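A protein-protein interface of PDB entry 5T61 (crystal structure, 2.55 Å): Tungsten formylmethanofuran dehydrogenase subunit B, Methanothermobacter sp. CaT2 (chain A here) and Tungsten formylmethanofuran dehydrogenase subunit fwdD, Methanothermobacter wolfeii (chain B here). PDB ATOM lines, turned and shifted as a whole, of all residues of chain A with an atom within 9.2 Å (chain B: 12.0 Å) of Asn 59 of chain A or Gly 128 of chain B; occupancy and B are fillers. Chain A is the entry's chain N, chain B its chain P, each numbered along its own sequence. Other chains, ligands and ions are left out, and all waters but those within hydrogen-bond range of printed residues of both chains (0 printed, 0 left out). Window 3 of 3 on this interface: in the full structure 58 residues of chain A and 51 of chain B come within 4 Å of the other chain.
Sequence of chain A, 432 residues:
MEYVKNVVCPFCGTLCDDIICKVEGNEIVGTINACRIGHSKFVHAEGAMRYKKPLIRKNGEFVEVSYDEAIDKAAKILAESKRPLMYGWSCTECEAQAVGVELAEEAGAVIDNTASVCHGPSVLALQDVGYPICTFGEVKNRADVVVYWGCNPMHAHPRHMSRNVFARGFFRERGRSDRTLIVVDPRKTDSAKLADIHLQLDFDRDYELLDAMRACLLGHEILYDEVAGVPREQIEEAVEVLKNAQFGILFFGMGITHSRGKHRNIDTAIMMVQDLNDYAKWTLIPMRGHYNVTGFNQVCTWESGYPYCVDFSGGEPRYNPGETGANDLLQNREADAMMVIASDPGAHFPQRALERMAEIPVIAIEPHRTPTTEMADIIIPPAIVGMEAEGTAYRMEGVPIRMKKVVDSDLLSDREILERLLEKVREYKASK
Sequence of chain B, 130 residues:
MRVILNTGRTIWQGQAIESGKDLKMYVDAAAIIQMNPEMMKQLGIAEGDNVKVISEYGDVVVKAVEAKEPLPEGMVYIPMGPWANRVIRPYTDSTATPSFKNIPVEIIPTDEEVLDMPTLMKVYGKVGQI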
ATOM      1  N   ILE A  56       7.263  -1.522 -27.871  1.00  0.00           N
ATOM      2  CA  ILE A  56       8.058  -0.693 -26.980  1.00  0.00           C
ATOM      3  C   ILE A  56       9.524  -0.959 -27.273  1.00  0.00           C
ATOM      4  O   ILE A  56       9.920  -2.093 -27.569  1.00  0.00           O
ATOM      5  CB  ILE A  56       7.733  -0.944 -25.490  1.00  0.00           C
ATOM      6  CG1 ILE A  56       6.262  -0.637 -25.211  1.00  0.00           C
ATOM      7  CG2 ILE A  56       8.504   0.019 -24.624  1.00  0.00           C
ATOM      8  CD1 ILE A  56       5.876  -0.722 -23.741  1.00  0.00           C
ATOM      9  N   ARG A  57      10.326   0.096 -27.214  1.00  0.00           N
ATOM     10  CA  ARG A  57      11.758  -0.004 -27.433  1.00  0.00           C
ATOM     11  C   ARG A  57      12.405  -0.290 -26.083  1.00  0.00           C
ATOM     12  O   ARG A  57      12.291   0.522 -25.158  1.00  0.00           O
ATOM     13  CB  ARG A  57      12.302   1.295 -28.015  1.00  0.00           C
ATOM     14  CG  ARG A  57      13.687   1.182 -28.620  1.00  0.00           C
ATOM     15  CD  ARG A  57      14.243   2.549 -29.055  1.00  0.00           C
ATOM     16  NE  ARG A  57      13.399   3.348 -29.946  1.00  0.00           N
ATOM     17  CZ  ARG A  57      13.903   4.130 -30.897  1.00  0.00           C
ATOM     18  NH1 ARG A  57      15.231   4.206 -31.079  1.00  0.00           N
ATOM     19  NH2 ARG A  57      13.118   4.871 -31.681  1.00  0.00           N
ATOM     20  N   LYS A  58      13.050  -1.444 -25.964  1.00  0.00           N
ATOM     21  CA  LYS A  58      13.798  -1.795 -24.760  1.00  0.00           C
ATOM     22  C   LYS A  58      15.268  -1.553 -25.069  1.00  0.00           C
ATOM     23  O   LYS A  58      15.938  -2.396 -25.674  1.00  0.00           O
ATOM     24  CB  LYS A  58      13.519  -3.234 -24.338  1.00  0.00           C
ATOM     25  CG  LYS A  58      12.051  -3.600 -24.432  1.00  0.00           C
ATOM     26  CD  LYS A  58      11.311  -3.467 -23.108  1.00  0.00           C
ATOM     27  CE  LYS A  58       9.814  -3.700 -23.295  1.00  0.00           C
ATOM     28  NZ  LYS A  58       9.208  -4.558 -22.239  1.00  0.00           N
ATOM     29  N   ASN A  59      15.755  -0.386 -24.644  1.00  0.00           N
ATOM     30  CA  ASN A  59      17.036   0.168 -25.063  1.00  0.00           C
ATOM     31  C   ASN A  59      17.084   0.348 -26.576  1.00  0.00           C
ATOM     32  O   ASN A  59      16.757   1.426 -27.082  1.00  0.00           O
ATOM     33  CB  ASN A  59      18.198  -0.702 -24.592  1.00  0.00           C
ATOM     34  CG  ASN A  59      18.246  -0.857 -23.078  1.00  0.00           C
ATOM     35  OD1 ASN A  59      17.243  -0.689 -22.387  1.00  0.00           O
ATOM     36  ND2 ASN A  59      19.420  -1.190 -22.561  1.00  0.00           N
ATOM     37  N   GLY A  60      17.470  -0.687 -27.312  1.00  0.00           N
ATOM     38  CA  GLY A  60      17.669  -0.496 -28.733  1.00  0.00           C
ATOM     39  C   GLY A  60      16.869  -1.375 -29.670  1.00  0.00           C
ATOM     40  O   GLY A  60      17.109  -1.348 -30.878  1.00  0.00           O
ATOM     41  N   GLU A  61      15.919  -2.153 -29.154  1.00  0.00           N
ATOM     42  CA  GLU A  61      15.213  -3.128 -29.981  1.00  0.00           C
ATOM     43  C   GLU A  61      13.730  -3.153 -29.636  1.00  0.00           C
ATOM     44  O   GLU A  61      13.364  -3.260 -28.460  1.00  0.00           O
ATOM     45  CB  GLU A  61      15.839  -4.522 -29.813  1.00  0.00           C
ATOM     46  CG  GLU A  61      17.323  -4.616 -30.236  1.00  0.00           C
ATOM     47  CD  GLU A  61      18.274  -4.256 -29.112  1.00  0.00           C
ATOM     48  OE1 GLU A  61      17.960  -4.535 -27.947  1.00  0.00           O
ATOM     49  OE2 GLU A  61      19.344  -3.690 -29.384  1.00  0.00           O
ATOM     50  N   PHE A  62      12.883  -3.068 -30.660  1.00  0.00           N
ATOM     51  CA  PHE A  62      11.441  -3.045 -30.463  1.00  0.00           C
ATOM     52  C   PHE A  62      10.899  -4.438 -30.169  1.00  0.00           C
ATOM     53  O   PHE A  62      11.285  -5.421 -30.809  1.00  0.00           O
ATOM     54  CB  PHE A  62      10.744  -2.478 -31.699  1.00  0.00           C
ATOM     55  CG  PHE A  62      10.868  -0.988 -31.837  1.00  0.00           C
ATOM     56  CD1 PHE A  62      10.027  -0.149 -31.126  1.00  0.00           C
ATOM     57  CD2 PHE A  62      11.814  -0.425 -32.679  1.00  0.00           C
ATOM     58  CE1 PHE A  62      10.127   1.221 -31.244  1.00  0.00           C
ATOM     59  CE2 PHE A  62      11.920   0.949 -32.802  1.00  0.00           C
ATOM     60  CZ  PHE A  62      11.075   1.772 -32.085  1.00  0.00           C
ATOM     61  N   VAL A  63       9.995  -4.510 -29.196  1.00  0.00           N
ATOM     62  CA  VAL A  63       9.340  -5.748 -28.799  1.00  0.00           C
ATOM     63  C   VAL A  63       7.842  -5.495 -28.700  1.00  0.00           C
ATOM     64  O   VAL A  63       7.409  -4.429 -28.244  1.00  0.00           O
ATOM     65  CB  VAL A  63       9.906  -6.284 -27.466  1.00  0.00           C
ATOM     66  CG1 VAL A  63       9.809  -5.220 -26.419  1.00  0.00           C
ATOM     67  CG2 VAL A  63       9.167  -7.537 -27.019  1.00  0.00           C
ATOM     68  N   MET A 357      13.719  15.495 -29.792  1.00  0.00           N
ATOM     69  CA  MET A 357      12.967  14.249 -29.745  1.00  0.00           C
ATOM     70  C   MET A 357      13.883  13.065 -29.502  1.00  0.00           C
ATOM     71  O   MET A 357      13.462  12.070 -28.905  1.00  0.00           O
ATOM     72  CB  MET A 357      12.174  14.051 -31.041  1.00  0.00           C
ATOM     73  CG  MET A 357      10.849  14.796 -31.098  1.00  0.00           C
ATOM     74  SD  MET A 357      10.126  14.745 -32.753  1.00  0.00           S
ATOM     75  CE  MET A 357       9.495  13.069 -32.815  1.00  0.00           C
ATOM     76  N   ALA A 358      15.139  13.166 -29.933  1.00  0.00           N
ATOM     77  CA  ALA A 358      16.107  12.106 -29.697  1.00  0.00           C
ATOM     78  C   ALA A 358      16.441  11.950 -28.220  1.00  0.00           C
ATOM     79  O   ALA A 358      16.929  10.888 -27.822  1.00  0.00           O
ATOM     80  CB  ALA A 358      17.384  12.373 -30.495  1.00  0.00           C
ATOM     81  N   GLU A 359      16.194  12.977 -27.405  1.00  0.00           N
ATOM     82  CA  GLU A 359      16.625  13.002 -26.012  1.00  0.00           C
ATOM     83  C   GLU A 359      15.517  12.695 -25.013  1.00  0.00           C
ATOM     84  O   GLU A 359      15.795  12.644 -23.811  1.00  0.00           O
ATOM     85  CB  GLU A 359      17.197  14.379 -25.660  1.00  0.00           C
ATOM     86  CG  GLU A 359      18.238  14.936 -26.598  1.00  0.00           C
ATOM     87  CD  GLU A 359      18.685  16.316 -26.162  1.00  0.00           C
ATOM     88  OE1 GLU A 359      19.780  16.436 -25.575  1.00  0.00           O
ATOM     89  OE2 GLU A 359      17.924  17.284 -26.383  1.00  0.00           O
ATOM     90  N   ILE A 360      14.277  12.514 -25.456  1.00  0.00           N
ATOM     91  CA  ILE A 360      13.146  12.498 -24.529  1.00  0.00           C
ATOM     92  C   ILE A 360      12.231  11.325 -24.849  1.00  0.00           C
ATOM     93  O   ILE A 360      12.275  10.763 -25.952  1.00  0.00           O
ATOM     94  CB  ILE A 360      12.347  13.818 -24.574  1.00  0.00           C
ATOM     95  CG1 ILE A 360      11.788  14.056 -25.975  1.00  0.00           C
ATOM     96  CG2 ILE A 360      13.199  14.987 -24.079  1.00  0.00           C
ATOM     97  CD1 ILE A 360      10.825  15.205 -26.039  1.00  0.00           C
ATOM     98  N   PRO A 361      11.392  10.925 -23.888  1.00  0.00           N
ATOM     99  CA  PRO A 361      10.405   9.870 -24.173  1.00  0.00           C
ATOM    100  C   PRO A 361       9.393  10.343 -25.207  1.00  0.00           C
ATOM    101  O   PRO A 361       8.792  11.411 -25.067  1.00  0.00           O
ATOM    102  CB  PRO A 361       9.741   9.606 -22.815  1.00  0.00           C
ATOM    103  CG  PRO A 361      10.472  10.401 -21.809  1.00  0.00           C
ATOM    104  CD  PRO A 361      11.336  11.397 -22.492  1.00  0.00           C
ATOM    105  N   VAL A 362       9.218   9.543 -26.255  1.00  0.00           N
ATOM    106  CA  VAL A 362       8.280   9.836 -27.331  1.00  0.00           C
ATOM    107  C   VAL A 362       7.258   8.710 -27.384  1.00  0.00           C
ATOM    108  O   VAL A 362       7.623   7.541 -27.563  1.00  0.00           O
ATOM    109  CB  VAL A 362       8.989   9.991 -28.684  1.00  0.00           C
ATOM    110  CG1 VAL A 362       7.976   9.941 -29.823  1.00  0.00           C
ATOM    111  CG2 VAL A 362       9.801  11.279 -28.720  1.00  0.00           C
ATOM    112  N   GLU A 374      10.209   5.730 -35.891  1.00  0.00           N
ATOM    113  CA  GLU A 374      11.643   5.484 -35.789  1.00  0.00           C
ATOM    114  C   GLU A 374      12.288   6.288 -34.665  1.00  0.00           C
ATOM    115  O   GLU A 374      13.387   5.939 -34.226  1.00  0.00           O
ATOM    116  CB  GLU A 374      12.334   5.809 -37.109  1.00  0.00           C
ATOM    117  CG  GLU A 374      11.861   4.975 -38.287  1.00  0.00           C
ATOM    118  CD  GLU A 374      12.593   3.655 -38.387  1.00  0.00           C
ATOM    119  OE1 GLU A 374      13.774   3.602 -37.974  1.00  0.00           O
ATOM    120  OE2 GLU A 374      11.996   2.681 -38.896  1.00  0.00           O
ATOM    121  N   MET A 375      11.630   7.347 -34.192  1.00  0.00           N
ATOM    122  CA  MET A 375      12.089   8.112 -33.040  1.00  0.00           C
ATOM    123  C   MET A 375      11.257   7.849 -31.793  1.00  0.00           C
ATOM    124  O   MET A 375      11.397   8.580 -30.808  1.00  0.00           O
ATOM    125  CB  MET A 375      12.063   9.615 -33.345  1.00  0.00           C
ATOM    126  CG  MET A 375      12.814  10.051 -34.586  1.00  0.00           C
ATOM    127  SD  MET A 375      14.595  10.055 -34.325  1.00  0.00           S
ATOM    128  CE  MET A 375      14.738  11.280 -33.022  1.00  0.00           C
ATOM    129  N   ALA A 376      10.406   6.831 -31.800  1.00  0.00           N
ATOM    130  CA  ALA A 376       9.460   6.622 -30.716  1.00  0.00           C
ATOM    131  C   ALA A 376       9.966   5.575 -29.731  1.00  0.00           C
ATOM    132  O   ALA A 376      10.748   4.688 -30.080  1.00  0.00           O
ATOM    133  CB  ALA A 376       8.090   6.203 -31.253  1.00  0.00           C
ATOM    134  N   ASP A 377       9.509   5.698 -28.488  1.00  0.00           N
ATOM    135  CA  ASP A 377       9.770   4.696 -27.464  1.00  0.00           C
ATOM    136  C   ASP A 377       8.611   3.728 -27.282  1.00  0.00           C
ATOM    137  O   ASP A 377       8.842   2.548 -26.998  1.00  0.00           O
ATOM    138  CB  ASP A 377      10.083   5.375 -26.126  1.00  0.00           C
ATOM    139  CG  ASP A 377      11.383   6.152 -26.160  1.00  0.00           C
ATOM    140  OD1 ASP A 377      12.458   5.515 -26.184  1.00  0.00           O
ATOM    141  OD2 ASP A 377      11.329   7.401 -26.161  1.00  0.00           O
ATOM    142  N   ILE A 378       7.375   4.200 -27.442  1.00  0.00           N
ATOM    143  CA  ILE A 378       6.181   3.370 -27.354  1.00  0.00           C
ATOM    144  C   ILE A 378       5.344   3.618 -28.601  1.00  0.00           C
ATOM    145  O   ILE A 378       5.118   4.773 -28.979  1.00  0.00           O
ATOM    146  CB  ILE A 378       5.362   3.679 -26.085  1.00  0.00           C
ATOM    147  CG1 ILE A 378       6.206   3.450 -24.829  1.00  0.00           C
ATOM    148  CG2 ILE A 378       4.110   2.819 -26.036  1.00  0.00           C
ATOM    149  CD1 ILE A 378       5.536   3.930 -23.559  1.00  0.00           C
ATOM    150  N   MET B 121      17.053   8.900 -40.411  1.00  0.00           N
ATOM    151  CA  MET B 121      16.669   9.268 -39.049  1.00  0.00           C
ATOM    152  C   MET B 121      17.769   8.993 -38.031  1.00  0.00           C
ATOM    153  O   MET B 121      17.817   9.657 -36.989  1.00  0.00           O
ATOM    154  CB  MET B 121      15.390   8.533 -38.651  1.00  0.00           C
ATOM    155  CG  MET B 121      14.183   8.829 -39.533  1.00  0.00           C
ATOM    156  SD  MET B 121      13.737  10.578 -39.561  1.00  0.00           S
ATOM    157  CE  MET B 121      14.542  11.095 -41.065  1.00  0.00           C
ATOM    158  N   LYS B 122      18.659   8.036 -38.303  1.00  0.00           N
ATOM    159  CA  LYS B 122      19.722   7.732 -37.347  1.00  0.00           C
ATOM    160  C   LYS B 122      20.687   8.900 -37.172  1.00  0.00           C
ATOM    161  O   LYS B 122      21.395   8.956 -36.160  1.00  0.00           O
ATOM    162  CB  LYS B 122      20.445   6.449 -37.773  1.00  0.00           C
ATOM    163  CG  LYS B 122      19.466   5.286 -37.898  1.00  0.00           C
ATOM    164  CD  LYS B 122      19.335   4.536 -36.573  1.00  0.00           C
ATOM    165  CE  LYS B 122      18.087   3.647 -36.564  1.00  0.00           C
ATOM    166  NZ  LYS B 122      17.878   2.832 -37.797  1.00  0.00           N
ATOM    167  N   TYR B 124      19.970  11.708 -36.241  1.00  0.00           N
ATOM    168  CA  TYR B 124      19.586  12.403 -35.022  1.00  0.00           C
ATOM    169  C   TYR B 124      19.916  11.623 -33.754  1.00  0.00           C
ATOM    170  O   TYR B 124      19.849  12.197 -32.661  1.00  0.00           O
ATOM    171  CB  TYR B 124      18.096  12.746 -35.068  1.00  0.00           C
ATOM    172  CG  TYR B 124      17.756  13.678 -36.208  1.00  0.00           C
ATOM    173  CD1 TYR B 124      18.215  14.989 -36.214  1.00  0.00           C
ATOM    174  CD2 TYR B 124      16.987  13.249 -37.282  1.00  0.00           C
ATOM    175  CE1 TYR B 124      17.915  15.849 -37.253  1.00  0.00           C
ATOM    176  CE2 TYR B 124      16.682  14.104 -38.329  1.00  0.00           C
ATOM    177  CZ  TYR B 124      17.148  15.402 -38.308  1.00  0.00           C
ATOM    178  OH  TYR B 124      16.847  16.262 -39.340  1.00  0.00           O
ATOM    179  N   GLY B 125      20.277  10.344 -33.870  1.00  0.00           N
ATOM    180  CA  GLY B 125      20.840   9.597 -32.759  1.00  0.00           C
ATOM    181  C   GLY B 125      19.898   9.323 -31.605  1.00  0.00           C
ATOM    182  O   GLY B 125      20.191   9.694 -30.464  1.00  0.00           O
ATOM    183  N   LYS B 126      18.766   8.679 -31.886  1.00  0.00           N
ATOM    184  CA  LYS B 126      17.770   8.416 -30.852  1.00  0.00           C
ATOM    185  C   LYS B 126      18.339   7.520 -29.759  1.00  0.00           C
ATOM    186  O   LYS B 126      18.852   6.430 -30.030  1.00  0.00           O
ATOM    187  CB  LYS B 126      16.523   7.774 -31.465  1.00  0.00           C
ATOM    188  CG  LYS B 126      15.379   7.532 -30.469  1.00  0.00           C
ATOM    189  CD  LYS B 126      15.248   8.695 -29.487  1.00  0.00           C
ATOM    190  CE  LYS B 126      13.824   8.921 -28.999  1.00  0.00           C
ATOM    191  NZ  LYS B 126      13.307   7.862 -28.098  1.00  0.00           N
ATOM    192  N   VAL B 127      18.259   7.997 -28.518  1.00  0.00           N
ATOM    193  CA  VAL B 127      18.619   7.219 -27.341  1.00  0.00           C
ATOM    194  C   VAL B 127      17.335   6.724 -26.690  1.00  0.00           C
ATOM    195  O   VAL B 127      16.405   7.508 -26.463  1.00  0.00           O
ATOM    196  CB  VAL B 127      19.454   8.055 -26.355  1.00  0.00           C
ATOM    197  CG1 VAL B 127      19.713   7.274 -25.079  1.00  0.00           C
ATOM    198  CG2 VAL B 127      20.764   8.478 -26.996  1.00  0.00           C
ATOM    199  N   GLY B 128      17.284   5.430 -26.384  1.00  0.00           N
ATOM    200  CA  GLY B 128      16.091   4.860 -25.797  1.00  0.00           C
ATOM    201  C   GLY B 128      15.863   5.324 -24.372  1.00  0.00           C
ATOM    202  O   GLY B 128      16.774   5.776 -23.677  1.00  0.00           O
ATOM    203  N   GLN B 129      14.606   5.213 -23.942  1.00  0.00           N
ATOM    204  CA  GLN B 129      14.199   5.549 -22.576  1.00  0.00           C
ATOM    205  C   GLN B 129      12.761   5.108 -22.296  1.00  0.00           C
ATOM    206  O   GLN B 129      12.524   4.075 -21.665  1.00  0.00           O
ATOM    207  CB  GLN B 129      14.343   7.052 -22.319  1.00  0.00           C
ATOM    208  CG  GLN B 129      13.952   7.935 -23.494  1.00  0.00           C
ATOM    209  CD  GLN B 129      14.816   9.178 -23.583  1.00  0.00           C
ATOM    210  OE1 GLN B 129      14.836  10.001 -22.669  1.00  0.00           O
ATOM    211  NE2 GLN B 129      15.547   9.314 -24.685  1.00  0.00           N
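O of Ala 358 of chain A lies within hydrogen-bond range of N of Val 127 of chain B (3.3 Å). The side-chain amide oxygen of Gln 129 of chain B lies close to the backbone carbonyl oxygen of Glu 359 of chain A (3.0 Å). The backbone carbonyl oxygen (O) of Met 375 of chain A sits close to the side-chain amino group (NZ) of Lys 126 of chain B (3.4 Å). OD2 of Asp 377 of chain A lies within salt-bridge range of NZ of Lys 126 of chain B (2.8 Å). The side-chain carboxylate (OD1) of Asp 377 of chain A sits at hydrogen-bond distance from the backbone NH (N) of Gln 129 of chain B, at 3.1 Å.
O of Glu 374 of chain A sits at hydrogen-bond distance from NH2 of Arg 57 of chain A (2.8 Å). The guanidinium group of Arg 57 of chain A is in hydrogen-bond range of the backbone carbonyl oxygen of Ala 376 of chain A (2.9 Å). O of Asp 377 of chain A is in hydrogen-bond range of N of Arg 57 of chain A (2.9 Å). The backbone carbonyl oxygen of Val 362 of chain A lies within hydrogen-bond range of the backbone NH of Asp 377 of chain A, 2.8 Å away. O of Val 127 of chain B sits at hydrogen-bond distance from NE2 of Gln 129 of chain B (2.7 Å).
Among the printed residues, merely in contact across the chains: Arg 57 of chain A with Lys 126 of chain B (3.4 Å), Asn 59 of chain A with Gly 128 of chain B (3.7 Å), Met 357 of chain A with Lys 126 of chain B (3.2 Å), Ala 358 of chain A with Tyr 124 of chain B (3.3 Å), Ala 358 of chain A with Gly 125 of chain B (3.9 Å), Ala 358 of chain A with Lys 126 of chain B (3.2 Å), Ala 358 of chain A with Gln 129 of chain B (3.8 Å), Ile 360 of chain A with Lys 126 of chain B (3.8 Å), Ile 360 of chain A with Gln 129 of chain B (3.5 Å), Pro 361 of chain A with Gln 129 of chain B (3.8 Å) and Asp 377 of chain A with Gly 128 of chain B (3.7 Å).
Of chain B, only Gly 128 comes within 4 Å of Asn 59 of chain A. Arg 57 of chain A touches just one residue of chain B: Lys 126 (3.4 Å). No residue of chain B comes within 4 Å of Gly 60 of chain A. Of the printed residues of chain A, Val 127 of chain B touches Ala 358. Gln 129 of chain B touches just these residues of chain A: Ala 358, Glu 359, Ile 360, Pro 361 and Asp 377. Printed residues of chain B within 4 Å of Pro 361 of chain A: Gln 129 (3.8 Å). Of the printed residues of chain B, Glu 359 of chain A touches Gln 129. Printed residues of chain B within 4 Å of Ile 360 of chain A: Lys 126 and Gln 129. Of the printed residues of chain A, Tyr 124 of chain B touches Ala 358 (3.3 Å). Of the printed residues of chain B, Met 375 of chain A touches Lys 126 (3.0 Å). Val 362 of chain A touches none of the printed residues of chain B. Phe 62 of chain A touches none of the printed residues of chain B. The nearest residue of chain A that does not touch Gly 128 of chain B is Arg 57 of chain A (4.4 Å).
Of the 19 printed residues of chain A, 9 touch a printed residue of chain B. Hydrophobic or aromatic side chains of chain A within 4 Å of the printed part of chain B: Ala 358 and Pro 361. Of the 8 printed residues of chain B, 6 touch a printed residue of chain A. Among the printed residues, Asp or Glu carboxylates within 4 Å of a Lys or Arg side-chain nitrogen of the other chain: Asp 377 of chain A with Lys 126 of chain B (2.8 Å).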
